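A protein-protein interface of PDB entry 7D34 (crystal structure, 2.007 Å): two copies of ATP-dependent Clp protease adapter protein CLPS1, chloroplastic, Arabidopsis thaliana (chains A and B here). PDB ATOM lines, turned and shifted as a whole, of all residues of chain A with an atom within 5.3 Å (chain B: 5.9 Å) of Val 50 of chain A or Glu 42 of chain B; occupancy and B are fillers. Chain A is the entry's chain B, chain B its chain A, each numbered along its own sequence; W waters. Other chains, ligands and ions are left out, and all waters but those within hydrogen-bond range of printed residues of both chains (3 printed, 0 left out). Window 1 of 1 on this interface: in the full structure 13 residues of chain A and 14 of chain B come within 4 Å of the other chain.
Water W1 lies within hydrogen-bond range of the side-chain amide oxygen (OE1) of Gln 41 of chain B (2.6 Å), the side-chain amide nitrogen (ND2) of Asn 38 of chain A (2.6 Å) and the side-chain amide oxygen (OD1) of Asn 38 of chain B (3.2 Å).
Water W2 bridges the backbone NH (N) of Val 50 of chain A (2.8 Å) and the backbone NH (N) of Val 50 of chain B (3.3 Å).
Water W3 bridges N of Val 53 of chain A (3.0 Å) and O of Asn 46 of chain B (3.3 Å).
The side-chain carboxylate (OE1) of Glu 42 of chain B is in hydrogen-bond range of the side-chain amide nitrogen (ND2) of Asn 46 of chain B (3.3 Å).
O of Val 7 of chain A sits at hydrogen-bond distance from N of Val 51 of chain A (2.8 Å).
O of Ile 52 of chain A sits at hydrogen-bond distance from N of Val 7 of chain A (3.0 Å).
Along chain A the printed residues that touch a printed residue of chain B span positions 6 to 53.
Of the 14 printed residues of chain B, 7 touch a printed residue of chain A.
Among the printed residues, 17 pairs touch across the chains.
Among the printed residues, no Asp or Glu carboxylate lies within 4 Å of a Lys or Arg side-chain nitrogen of the other chain.
Val 50 of chain A touches just these residues of chain B: Glu 42 (3.9 Å), Asn 46 (3.9 Å) and Leu 48 (3.9 Å).
Of the printed residues of chain A, Asn 46 of chain B touches Asn 35 (3.6 Å), Val 50 (3.9 Å), Val 51 (2.6 Å), Ile 52 (3.4 Å) and Val 53 (3.7 Å).
Printed residues of chain A within 4 Å of Leu 48 of chain B: Arg 6 (3.2 Å), Val 50 (3.9 Å) and Val 53 (3.5 Å).
The nearest residue of chain B that does not touch Val 50 of chain A is Val 50 of chain B (4.9 Å).
The nearest printed residue of chain A that does not touch Gln 41 of chain B is Asn 35 of chain A (5.8 Å).
The side-chain amide oxygen of Asn 38 of chain B sits at hydrogen-bond distance from the side-chain amide nitrogen of Asn 38 of chain A, at 3.4 Å.
The side-chain amide nitrogen (ND2) of Asn 38 of chain B lies close to the side-chain carboxylate (OE2) of Glu 42 of chain A.
The side-chain amide oxygen of Gln 41 of chain B sits close to the side-chain amide oxygen of Asn 38 of chain A (2.9 Å).
The side-chain amide oxygen (OD1) of Asn 35 of chain A lies close to the side-chain carboxylate (OE2) of Glu 42 of chain B (2.9 Å).
O of Val 51 of chain A sits close to OD1 of Asn 46 of chain B (2.6 Å).
Asn 38 of chain B touches its own counterpart, Asn 38 of chain A.
Asn 38 of chain A touches Glu 42 of chain B, and with the chains exchanged Glu 42 of chain A touches Asn 38 of chain B.
Val 50 of chain A touches Glu 42 of chain B, but with the chains exchanged Glu 42 of chain A does not touch Val 50 of chain B (4.2 Å).
Val 50 of chain A touches Leu 48 of chain B, but with the chains exchanged Leu 48 of chain A does not touch Val 50 of chain B (4.4 Å).
Among the printed residues, merely in contact across the chains: Arg 6 of chain A with Leu 48 of chain B (3.2 Å), Asn 35 of chain A with Ile 45 of chain B (3.6 Å), Asn 35 of chain A with Asn 46 of chain B (3.6 Å), Asn 38 of chain A with Glu 42 of chain B (3.1 Å), Ile 39 of chain A with Glu 42 of chain B (3.3 Å), Glu 42 of chain A with Ile 39 of chain B (3.6 Å), Val 50 of chain A with Glu 42 of chain B (3.9 Å), Val 50 of chain A with Asn 46 of chain B (3.9 Å), Val 50 of chain A with Leu 48 of chain B (3.9 Å), Ile 52 of chain A with Asn 46 of chain B (3.4 Å), Val 53 of chain A with Asn 46 of chain B (3.7 Å) and Val 53 of chain A with Leu 48 of chain B (3.5 Å).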
ATOM      1  N   ARG A   6     -36.815 -32.179   7.676  1.00  0.00           N
ATOM      2  CA  ARG A   6     -36.033 -31.149   7.016  1.00  0.00           C
ATOM      3  C   ARG A   6     -35.925 -29.947   7.942  1.00  0.00           C
ATOM      4  O   ARG A   6     -36.930 -29.489   8.495  1.00  0.00           O
ATOM      5  CB  ARG A   6     -36.663 -30.815   5.657  1.00  0.00           C
ATOM      6  CG  ARG A   6     -36.240 -31.829   4.589  1.00  0.00           C
ATOM      7  CD  ARG A   6     -37.176 -32.052   3.393  1.00  0.00           C
ATOM      8  NE  ARG A   6     -38.139 -30.993   3.109  1.00  0.00           N
ATOM      9  CZ  ARG A   6     -38.943 -31.028   2.052  1.00  0.00           C
ATOM     10  NH1 ARG A   6     -39.805 -30.059   1.819  1.00  0.00           N
ATOM     11  NH2 ARG A   6     -38.875 -32.050   1.217  1.00  0.00           N
ATOM     12  N   VAL A   7     -34.705 -29.455   8.127  1.00  0.00           N
ATOM     13  CA  VAL A   7     -34.489 -28.186   8.810  1.00  0.00           C
ATOM     14  C   VAL A   7     -34.494 -27.113   7.736  1.00  0.00           C
ATOM     15  O   VAL A   7     -33.673 -27.146   6.815  1.00  0.00           O
ATOM     16  CB  VAL A   7     -33.170 -28.175   9.597  1.00  0.00           C
ATOM     17  CG1 VAL A   7     -32.907 -26.778  10.172  1.00  0.00           C
ATOM     18  CG2 VAL A   7     -33.204 -29.199  10.730  1.00  0.00           C
ATOM     19  N   ILE A   8     -35.417 -26.172   7.841  1.00  0.00           N
ATOM     20  CA  ILE A   8     -35.574 -25.145   6.823  1.00  0.00           C
ATOM     21  C   ILE A   8     -34.971 -23.863   7.366  1.00  0.00           C
ATOM     22  O   ILE A   8     -35.119 -23.527   8.544  1.00  0.00           O
ATOM     23  CB  ILE A   8     -37.052 -24.939   6.426  1.00  0.00           C
ATOM     24  CG1 ILE A   8     -37.677 -26.248   5.940  1.00  0.00           C
ATOM     25  CG2 ILE A   8     -37.178 -23.851   5.353  1.00  0.00           C
ATOM     26  CD1 ILE A   8     -36.903 -26.929   4.825  1.00  0.00           C
ATOM     27  N   LEU A   9     -34.249 -23.157   6.510  1.00  0.00           N
ATOM     28  CA  LEU A   9     -33.798 -21.808   6.811  1.00  0.00           C
ATOM     29  C   LEU A   9     -34.564 -20.865   5.903  1.00  0.00           C
ATOM     30  O   LEU A   9     -34.474 -20.977   4.678  1.00  0.00           O
ATOM     31  CB  LEU A   9     -32.295 -21.635   6.585  1.00  0.00           C
ATOM     32  CG  LEU A   9     -31.686 -20.238   6.766  1.00  0.00           C
ATOM     33  CD1 LEU A   9     -31.663 -19.854   8.233  1.00  0.00           C
ATOM     34  CD2 LEU A   9     -30.290 -20.223   6.200  1.00  0.00           C
ATOM     35  N   ASN A  35     -20.705 -25.222   2.518  1.00  0.00           N
ATOM     36  CA  ASN A  35     -22.127 -25.551   2.548  1.00  0.00           C
ATOM     37  C   ASN A  35     -22.955 -24.404   3.129  1.00  0.00           C
ATOM     38  O   ASN A  35     -24.002 -24.042   2.578  1.00  0.00           O
ATOM     39  CB  ASN A  35     -22.332 -26.842   3.345  1.00  0.00           C
ATOM     40  CG  ASN A  35     -23.725 -27.412   3.183  1.00  0.00           C
ATOM     41  OD1 ASN A  35     -24.413 -27.154   2.192  1.00  0.00           O
ATOM     42  ND2 ASN A  35     -24.159 -28.176   4.170  1.00  0.00           N
ATOM     43  N   ASN A  38     -23.617 -21.555   0.699  1.00  0.00           N
ATOM     44  CA  ASN A  38     -24.623 -21.947  -0.284  1.00  0.00           C
ATOM     45  C   ASN A  38     -26.028 -21.819   0.290  1.00  0.00           C
ATOM     46  O   ASN A  38     -26.933 -21.286  -0.362  1.00  0.00           O
ATOM     47  CB  ASN A  38     -24.389 -23.385  -0.753  1.00  0.00           C
ATOM     48  CG  ASN A  38     -23.293 -23.499  -1.799  1.00  0.00           C
ATOM     49  OD1 ASN A  38     -22.812 -24.597  -2.088  1.00  0.00           O
ATOM     50  ND2 ASN A  38     -22.873 -22.366  -2.353  1.00  0.00           N
ATOM     51  N   ILE A  39     -26.227 -22.316   1.511  1.00  0.00           N
ATOM     52  CA  ILE A  39     -27.541 -22.251   2.147  1.00  0.00           C
ATOM     53  C   ILE A  39     -28.004 -20.803   2.247  1.00  0.00           C
ATOM     54  O   ILE A  39     -29.126 -20.458   1.856  1.00  0.00           O
ATOM     55  CB  ILE A  39     -27.488 -22.926   3.531  1.00  0.00           C
ATOM     56  CG1 ILE A  39     -27.061 -24.392   3.382  1.00  0.00           C
ATOM     57  CG2 ILE A  39     -28.856 -22.787   4.234  1.00  0.00           C
ATOM     58  CD1 ILE A  39     -26.899 -25.135   4.698  1.00  0.00           C
ATOM     59  N   GLU A  42     -28.963 -19.620  -1.145  1.00  0.00           N
ATOM     60  CA  GLU A  42     -30.196 -20.219  -1.642  1.00  0.00           C
ATOM     61  C   GLU A  42     -31.408 -19.766  -0.828  1.00  0.00           C
ATOM     62  O   GLU A  42     -32.475 -19.507  -1.396  1.00  0.00           O
ATOM     63  CB  GLU A  42     -30.061 -21.743  -1.632  1.00  0.00           C
ATOM     64  CG  GLU A  42     -29.196 -22.326  -2.750  1.00  0.00           C
ATOM     65  CD  GLU A  42     -29.436 -21.666  -4.091  1.00  0.00           C
ATOM     66  OE1 GLU A  42     -30.494 -21.944  -4.702  1.00  0.00           O
ATOM     67  OE2 GLU A  42     -28.573 -20.865  -4.517  1.00  0.00           O
ATOM     68  N   LEU A  48     -36.092 -19.650   1.171  1.00  0.00           N
ATOM     69  CA  LEU A  48     -35.918 -20.782   2.056  1.00  0.00           C
ATOM     70  C   LEU A  48     -34.945 -21.742   1.398  1.00  0.00           C
ATOM     71  O   LEU A  48     -34.868 -21.832   0.170  1.00  0.00           O
ATOM     72  CB  LEU A  48     -37.254 -21.479   2.335  1.00  0.00           C
ATOM     73  CG  LEU A  48     -37.779 -22.416   1.236  1.00  0.00           C
ATOM     74  CD1 LEU A  48     -38.986 -23.196   1.790  1.00  0.00           C
ATOM     75  CD2 LEU A  48     -38.084 -21.677  -0.086  1.00  0.00           C
ATOM     76  N   ALA A  49     -34.266 -22.510   2.242  1.00  0.00           N
ATOM     77  CA  ALA A  49     -33.248 -23.453   1.811  1.00  0.00           C
ATOM     78  C   ALA A  49     -33.148 -24.564   2.846  1.00  0.00           C
ATOM     79  O   ALA A  49     -33.319 -24.326   4.046  1.00  0.00           O
ATOM     80  CB  ALA A  49     -31.885 -22.764   1.643  1.00  0.00           C
ATOM     81  N   VAL A  50     -32.836 -25.766   2.376  1.00  0.00           N
ATOM     82  CA  VAL A  50     -32.715 -26.924   3.255  1.00  0.00           C
ATOM     83  C   VAL A  50     -31.353 -26.889   3.927  1.00  0.00           C
ATOM     84  O   VAL A  50     -30.320 -26.844   3.253  1.00  0.00           O
ATOM     85  CB  VAL A  50     -32.920 -28.225   2.475  1.00  0.00           C
ATOM     86  CG1 VAL A  50     -32.657 -29.434   3.332  1.00  0.00           C
ATOM     87  CG2 VAL A  50     -34.347 -28.266   1.993  1.00  0.00           C
ATOM     88  N   VAL A  51     -31.352 -26.906   5.253  1.00  0.00           N
ATOM     89  CA  VAL A  51     -30.112 -26.860   6.018  1.00  0.00           C
ATOM     90  C   VAL A  51     -29.530 -28.252   6.188  1.00  0.00           C
ATOM     91  O   VAL A  51     -28.348 -28.494   5.929  1.00  0.00           O
ATOM     92  CB  VAL A  51     -30.362 -26.186   7.383  1.00  0.00           C
ATOM     93  CG1 VAL A  51     -29.061 -26.180   8.218  1.00  0.00           C
ATOM     94  CG2 VAL A  51     -30.923 -24.781   7.191  1.00  0.00           C
ATOM     95  N   ILE A  52     -30.373 -29.185   6.620  1.00  0.00           N
ATOM     96  CA  ILE A  52     -29.952 -30.557   6.856  1.00  0.00           C
ATOM     97  C   ILE A  52     -31.205 -31.408   6.936  1.00  0.00           C
ATOM     98  O   ILE A  52     -32.292 -30.910   7.247  1.00  0.00           O
ATOM     99  CB  ILE A  52     -29.092 -30.680   8.141  1.00  0.00           C
ATOM    100  CG1 ILE A  52     -28.570 -32.104   8.298  1.00  0.00           C
ATOM    101  CG2 ILE A  52     -29.896 -30.329   9.387  1.00  0.00           C
ATOM    102  CD1 ILE A  52     -27.226 -32.234   8.977  1.00  0.00           C
ATOM    103  N   VAL A  53     -31.058 -32.694   6.638  1.00  0.00           N
ATOM    104  CA  VAL A  53     -32.119 -33.667   6.848  1.00  0.00           C
ATOM    105  C   VAL A  53     -31.625 -34.698   7.853  1.00  0.00           C
ATOM    106  O   VAL A  53     -30.517 -35.230   7.703  1.00  0.00           O
ATOM    107  CB  VAL A  53     -32.555 -34.343   5.535  1.00  0.00           C
ATOM    108  CG1 VAL A  53     -33.775 -35.249   5.793  1.00  0.00           C
ATOM    109  CG2 VAL A  53     -32.833 -33.307   4.453  1.00  0.00           C
ATOM    110  N   VAL B  37     -25.310 -24.235 -10.199  1.00  0.00           N
ATOM    111  CA  VAL B  37     -24.284 -24.985  -9.497  1.00  0.00           C
ATOM    112  C   VAL B  37     -24.621 -25.045  -8.021  1.00  0.00           C
ATOM    113  O   VAL B  37     -24.351 -26.051  -7.363  1.00  0.00           O
ATOM    114  CB  VAL B  37     -22.881 -24.382  -9.713  1.00  0.00           C
ATOM    115  CG1 VAL B  37     -22.390 -24.671 -11.142  1.00  0.00           C
ATOM    116  CG2 VAL B  37     -22.832 -22.878  -9.331  1.00  0.00           C
ATOM    117  N   ASN B  38     -25.196 -23.957  -7.464  1.00  0.00           N
ATOM    118  CA  ASN B  38     -25.596 -23.961  -6.052  1.00  0.00           C
ATOM    119  C   ASN B  38     -26.637 -25.032  -5.785  1.00  0.00           C
ATOM    120  O   ASN B  38     -26.532 -25.785  -4.811  1.00  0.00           O
ATOM    121  CB  ASN B  38     -26.162 -22.602  -5.591  1.00  0.00           C
ATOM    122  CG  ASN B  38     -25.071 -21.599  -5.241  1.00  0.00           C
ATOM    123  OD1 ASN B  38     -23.917 -21.834  -5.578  1.00  0.00           O
ATOM    124  ND2 ASN B  38     -25.420 -20.486  -4.568  1.00  0.00           N
ATOM    125  N   ILE B  39     -27.666 -25.083  -6.632  1.00  0.00           N
ATOM    126  CA  ILE B  39     -28.741 -26.055  -6.479  1.00  0.00           C
ATOM    127  C   ILE B  39     -28.179 -27.467  -6.573  1.00  0.00           C
ATOM    128  O   ILE B  39     -28.463 -28.325  -5.740  1.00  0.00           O
ATOM    129  CB  ILE B  39     -29.850 -25.797  -7.523  1.00  0.00           C
ATOM    130  CG1 ILE B  39     -30.440 -24.390  -7.342  1.00  0.00           C
ATOM    131  CG2 ILE B  39     -31.005 -26.802  -7.392  1.00  0.00           C
ATOM    132  CD1 ILE B  39     -31.462 -23.915  -8.385  1.00  0.00           C
ATOM    133  N   MET B  40     -27.400 -27.743  -7.606  1.00  0.00           N
ATOM    134  CA  MET B  40     -26.765 -29.046  -7.711  1.00  0.00           C
ATOM    135  C   MET B  40     -25.923 -29.385  -6.471  1.00  0.00           C
ATOM    136  O   MET B  40     -26.061 -30.478  -5.895  1.00  0.00           O
ATOM    137  CB  MET B  40     -25.949 -29.053  -8.984  1.00  0.00           C
ATOM    138  CG  MET B  40     -25.203 -30.344  -9.156  1.00  0.00           C
ATOM    139  SD  MET B  40     -23.582 -30.531  -8.376  1.00  0.00           S
ATOM    140  CE  MET B  40     -22.650 -29.234  -9.139  1.00  0.00           C
ATOM    141  N   GLN B  41     -25.084 -28.433  -6.024  1.00  0.00           N
ATOM    142  CA  GLN B  41     -24.266 -28.621  -4.824  1.00  0.00           C
ATOM    143  C   GLN B  41     -25.143 -28.968  -3.618  1.00  0.00           C
ATOM    144  O   GLN B  41     -24.891 -29.948  -2.904  1.00  0.00           O
ATOM    145  CB  GLN B  41     -23.447 -27.351  -4.567  1.00  0.00           C
ATOM    146  CG  GLN B  41     -22.074 -27.345  -5.281  1.00  0.00           C
ATOM    147  CD  GLN B  41     -21.464 -25.979  -5.362  1.00  0.00           C
ATOM    148  OE1 GLN B  41     -21.979 -25.035  -4.784  1.00  0.00           O
ATOM    149  NE2 GLN B  41     -20.363 -25.856  -6.102  1.00  0.00           N
ATOM    150  N   GLU B  42     -26.237 -28.225  -3.435  1.00  0.00           N
ATOM    151  CA  GLU B  42     -27.082 -28.392  -2.259  1.00  0.00           C
ATOM    152  C   GLU B  42     -27.813 -29.726  -2.269  1.00  0.00           C
ATOM    153  O   GLU B  42     -27.969 -30.355  -1.224  1.00  0.00           O
ATOM    154  CB  GLU B  42     -28.096 -27.254  -2.207  1.00  0.00           C
ATOM    155  CG  GLU B  42     -27.499 -25.974  -1.657  1.00  0.00           C
ATOM    156  CD  GLU B  42     -26.734 -26.200  -0.321  1.00  0.00           C
ATOM    157  OE1 GLU B  42     -27.388 -26.340   0.741  1.00  0.00           O
ATOM    158  OE2 GLU B  42     -25.477 -26.211  -0.336  1.00  0.00           O
ATOM    159  N   ALA B  43     -28.310 -30.160  -3.423  1.00  0.00           N
ATOM    160  CA  ALA B  43     -28.955 -31.471  -3.499  1.00  0.00           C
ATOM    161  C   ALA B  43     -27.951 -32.583  -3.247  1.00  0.00           C
ATOM    162  O   ALA B  43     -28.268 -33.582  -2.599  1.00  0.00           O
ATOM    163  CB  ALA B  43     -29.629 -31.649  -4.860  1.00  0.00           C
ATOM    164  N   HIS B  44     -26.734 -32.421  -3.758  1.00  0.00           N
ATOM    165  CA  HIS B  44     -25.693 -33.429  -3.574  1.00  0.00           C
ATOM    166  C   HIS B  44     -25.309 -33.583  -2.106  1.00  0.00           C
ATOM    167  O   HIS B  44     -25.114 -34.704  -1.622  1.00  0.00           O
ATOM    168  CB  HIS B  44     -24.456 -33.044  -4.403  1.00  0.00           C
ATOM    169  CG  HIS B  44     -23.289 -33.960  -4.213  1.00  0.00           C
ATOM    170  ND1 HIS B  44     -23.192 -35.183  -4.838  1.00  0.00           N
ATOM    171  CD2 HIS B  44     -22.175 -33.837  -3.459  1.00  0.00           C
ATOM    172  CE1 HIS B  44     -22.068 -35.776  -4.482  1.00  0.00           C
ATOM    173  NE2 HIS B  44     -21.431 -34.979  -3.645  1.00  0.00           N
ATOM    174  N   ILE B  45     -25.201 -32.474  -1.383  1.00  0.00           N
ATOM    175  CA  ILE B  45     -24.782 -32.504   0.014  1.00  0.00           C
ATOM    176  C   ILE B  45     -25.936 -32.844   0.946  1.00  0.00           C
ATOM    177  O   ILE B  45     -25.759 -33.586   1.915  1.00  0.00           O
ATOM    178  CB  ILE B  45     -24.135 -31.158   0.400  1.00  0.00           C
ATOM    179  CG1 ILE B  45     -22.739 -31.032  -0.224  1.00  0.00           C
ATOM    180  CG2 ILE B  45     -24.093 -30.999   1.919  1.00  0.00           C
ATOM    181  CD1 ILE B  45     -21.745 -31.970   0.350  1.00  0.00           C
ATOM    182  N   ASN B  46     -27.129 -32.318   0.679  1.00  0.00           N
ATOM    183  CA  ASN B  46     -28.247 -32.430   1.604  1.00  0.00           C
ATOM    184  C   ASN B  46     -29.293 -33.449   1.171  1.00  0.00           C
ATOM    185  O   ASN B  46     -30.216 -33.729   1.940  1.00  0.00           O
ATOM    186  CB  ASN B  46     -28.929 -31.062   1.750  1.00  0.00           C
ATOM    187  CG  ASN B  46     -28.186 -30.110   2.673  1.00  0.00           C
ATOM    188  OD1 ASN B  46     -28.390 -30.125   3.891  1.00  0.00           O
ATOM    189  ND2 ASN B  46     -27.295 -29.293   2.097  1.00  0.00           N
ATOM    190  N   GLY B  47     -29.173 -34.021  -0.027  1.00  0.00           N
ATOM    191  CA  GLY B  47     -30.164 -34.939  -0.540  1.00  0.00           C
ATOM    192  C   GLY B  47     -31.277 -34.291  -1.343  1.00  0.00           C
ATOM    193  O   GLY B  47     -31.950 -34.986  -2.112  1.00  0.00           O
ATOM    194  N   LEU B  48     -31.496 -32.987  -1.187  1.00  0.00           N
ATOM    195  CA  LEU B  48     -32.537 -32.288  -1.935  1.00  0.00           C
ATOM    196  C   LEU B  48     -32.251 -30.797  -1.903  1.00  0.00           C
ATOM    197  O   LEU B  48     -31.526 -30.308  -1.035  1.00  0.00           O
ATOM    198  CB  LEU B  48     -33.940 -32.563  -1.378  1.00  0.00           C
ATOM    199  CG  LEU B  48     -34.368 -31.867  -0.085  1.00  0.00           C
ATOM    200  CD1 LEU B  48     -35.873 -32.013   0.069  1.00  0.00           C
ATOM    201  CD2 LEU B  48     -33.684 -32.438   1.135  1.00  0.00           C
ATOM    202  N   ALA B  49     -32.824 -30.081  -2.865  1.00  0.00           N
ATOM    203  CA  ALA B  49     -32.639 -28.639  -2.917  1.00  0.00           C
ATOM    204  C   ALA B  49     -33.809 -27.979  -3.629  1.00  0.00           C
ATOM    205  O   ALA B  49     -34.403 -28.552  -4.543  1.00  0.00           O
ATOM    206  CB  ALA B  49     -31.324 -28.259  -3.616  1.00  0.00           C
ATOM    207  N   VAL B  50     -34.124 -26.760  -3.199  1.00  0.00           N
ATOM    208  CA  VAL B  50     -35.206 -25.983  -3.795  1.00  0.00           C
ATOM    209  C   VAL B  50     -34.691 -25.374  -5.091  1.00  0.00           C
ATOM    210  O   VAL B  50     -33.721 -24.608  -5.094  1.00  0.00           O
ATOM    211  CB  VAL B  50     -35.721 -24.897  -2.839  1.00  0.00           C
ATOM    212  CG1 VAL B  50     -36.707 -23.953  -3.568  1.00  0.00           C
ATOM    213  CG2 VAL B  50     -36.312 -25.577  -1.595  1.00  0.00           C
HETATM  214  O   HOH W   1     -21.144 -22.665  -4.266  1.00  0.00           O
HETATM  215  O   HOH W   2     -32.681 -25.517  -0.450  1.00  0.00           O
HETATM  216  O   HOH W   3     -28.700 -33.321   4.824  1.00  0.00           O
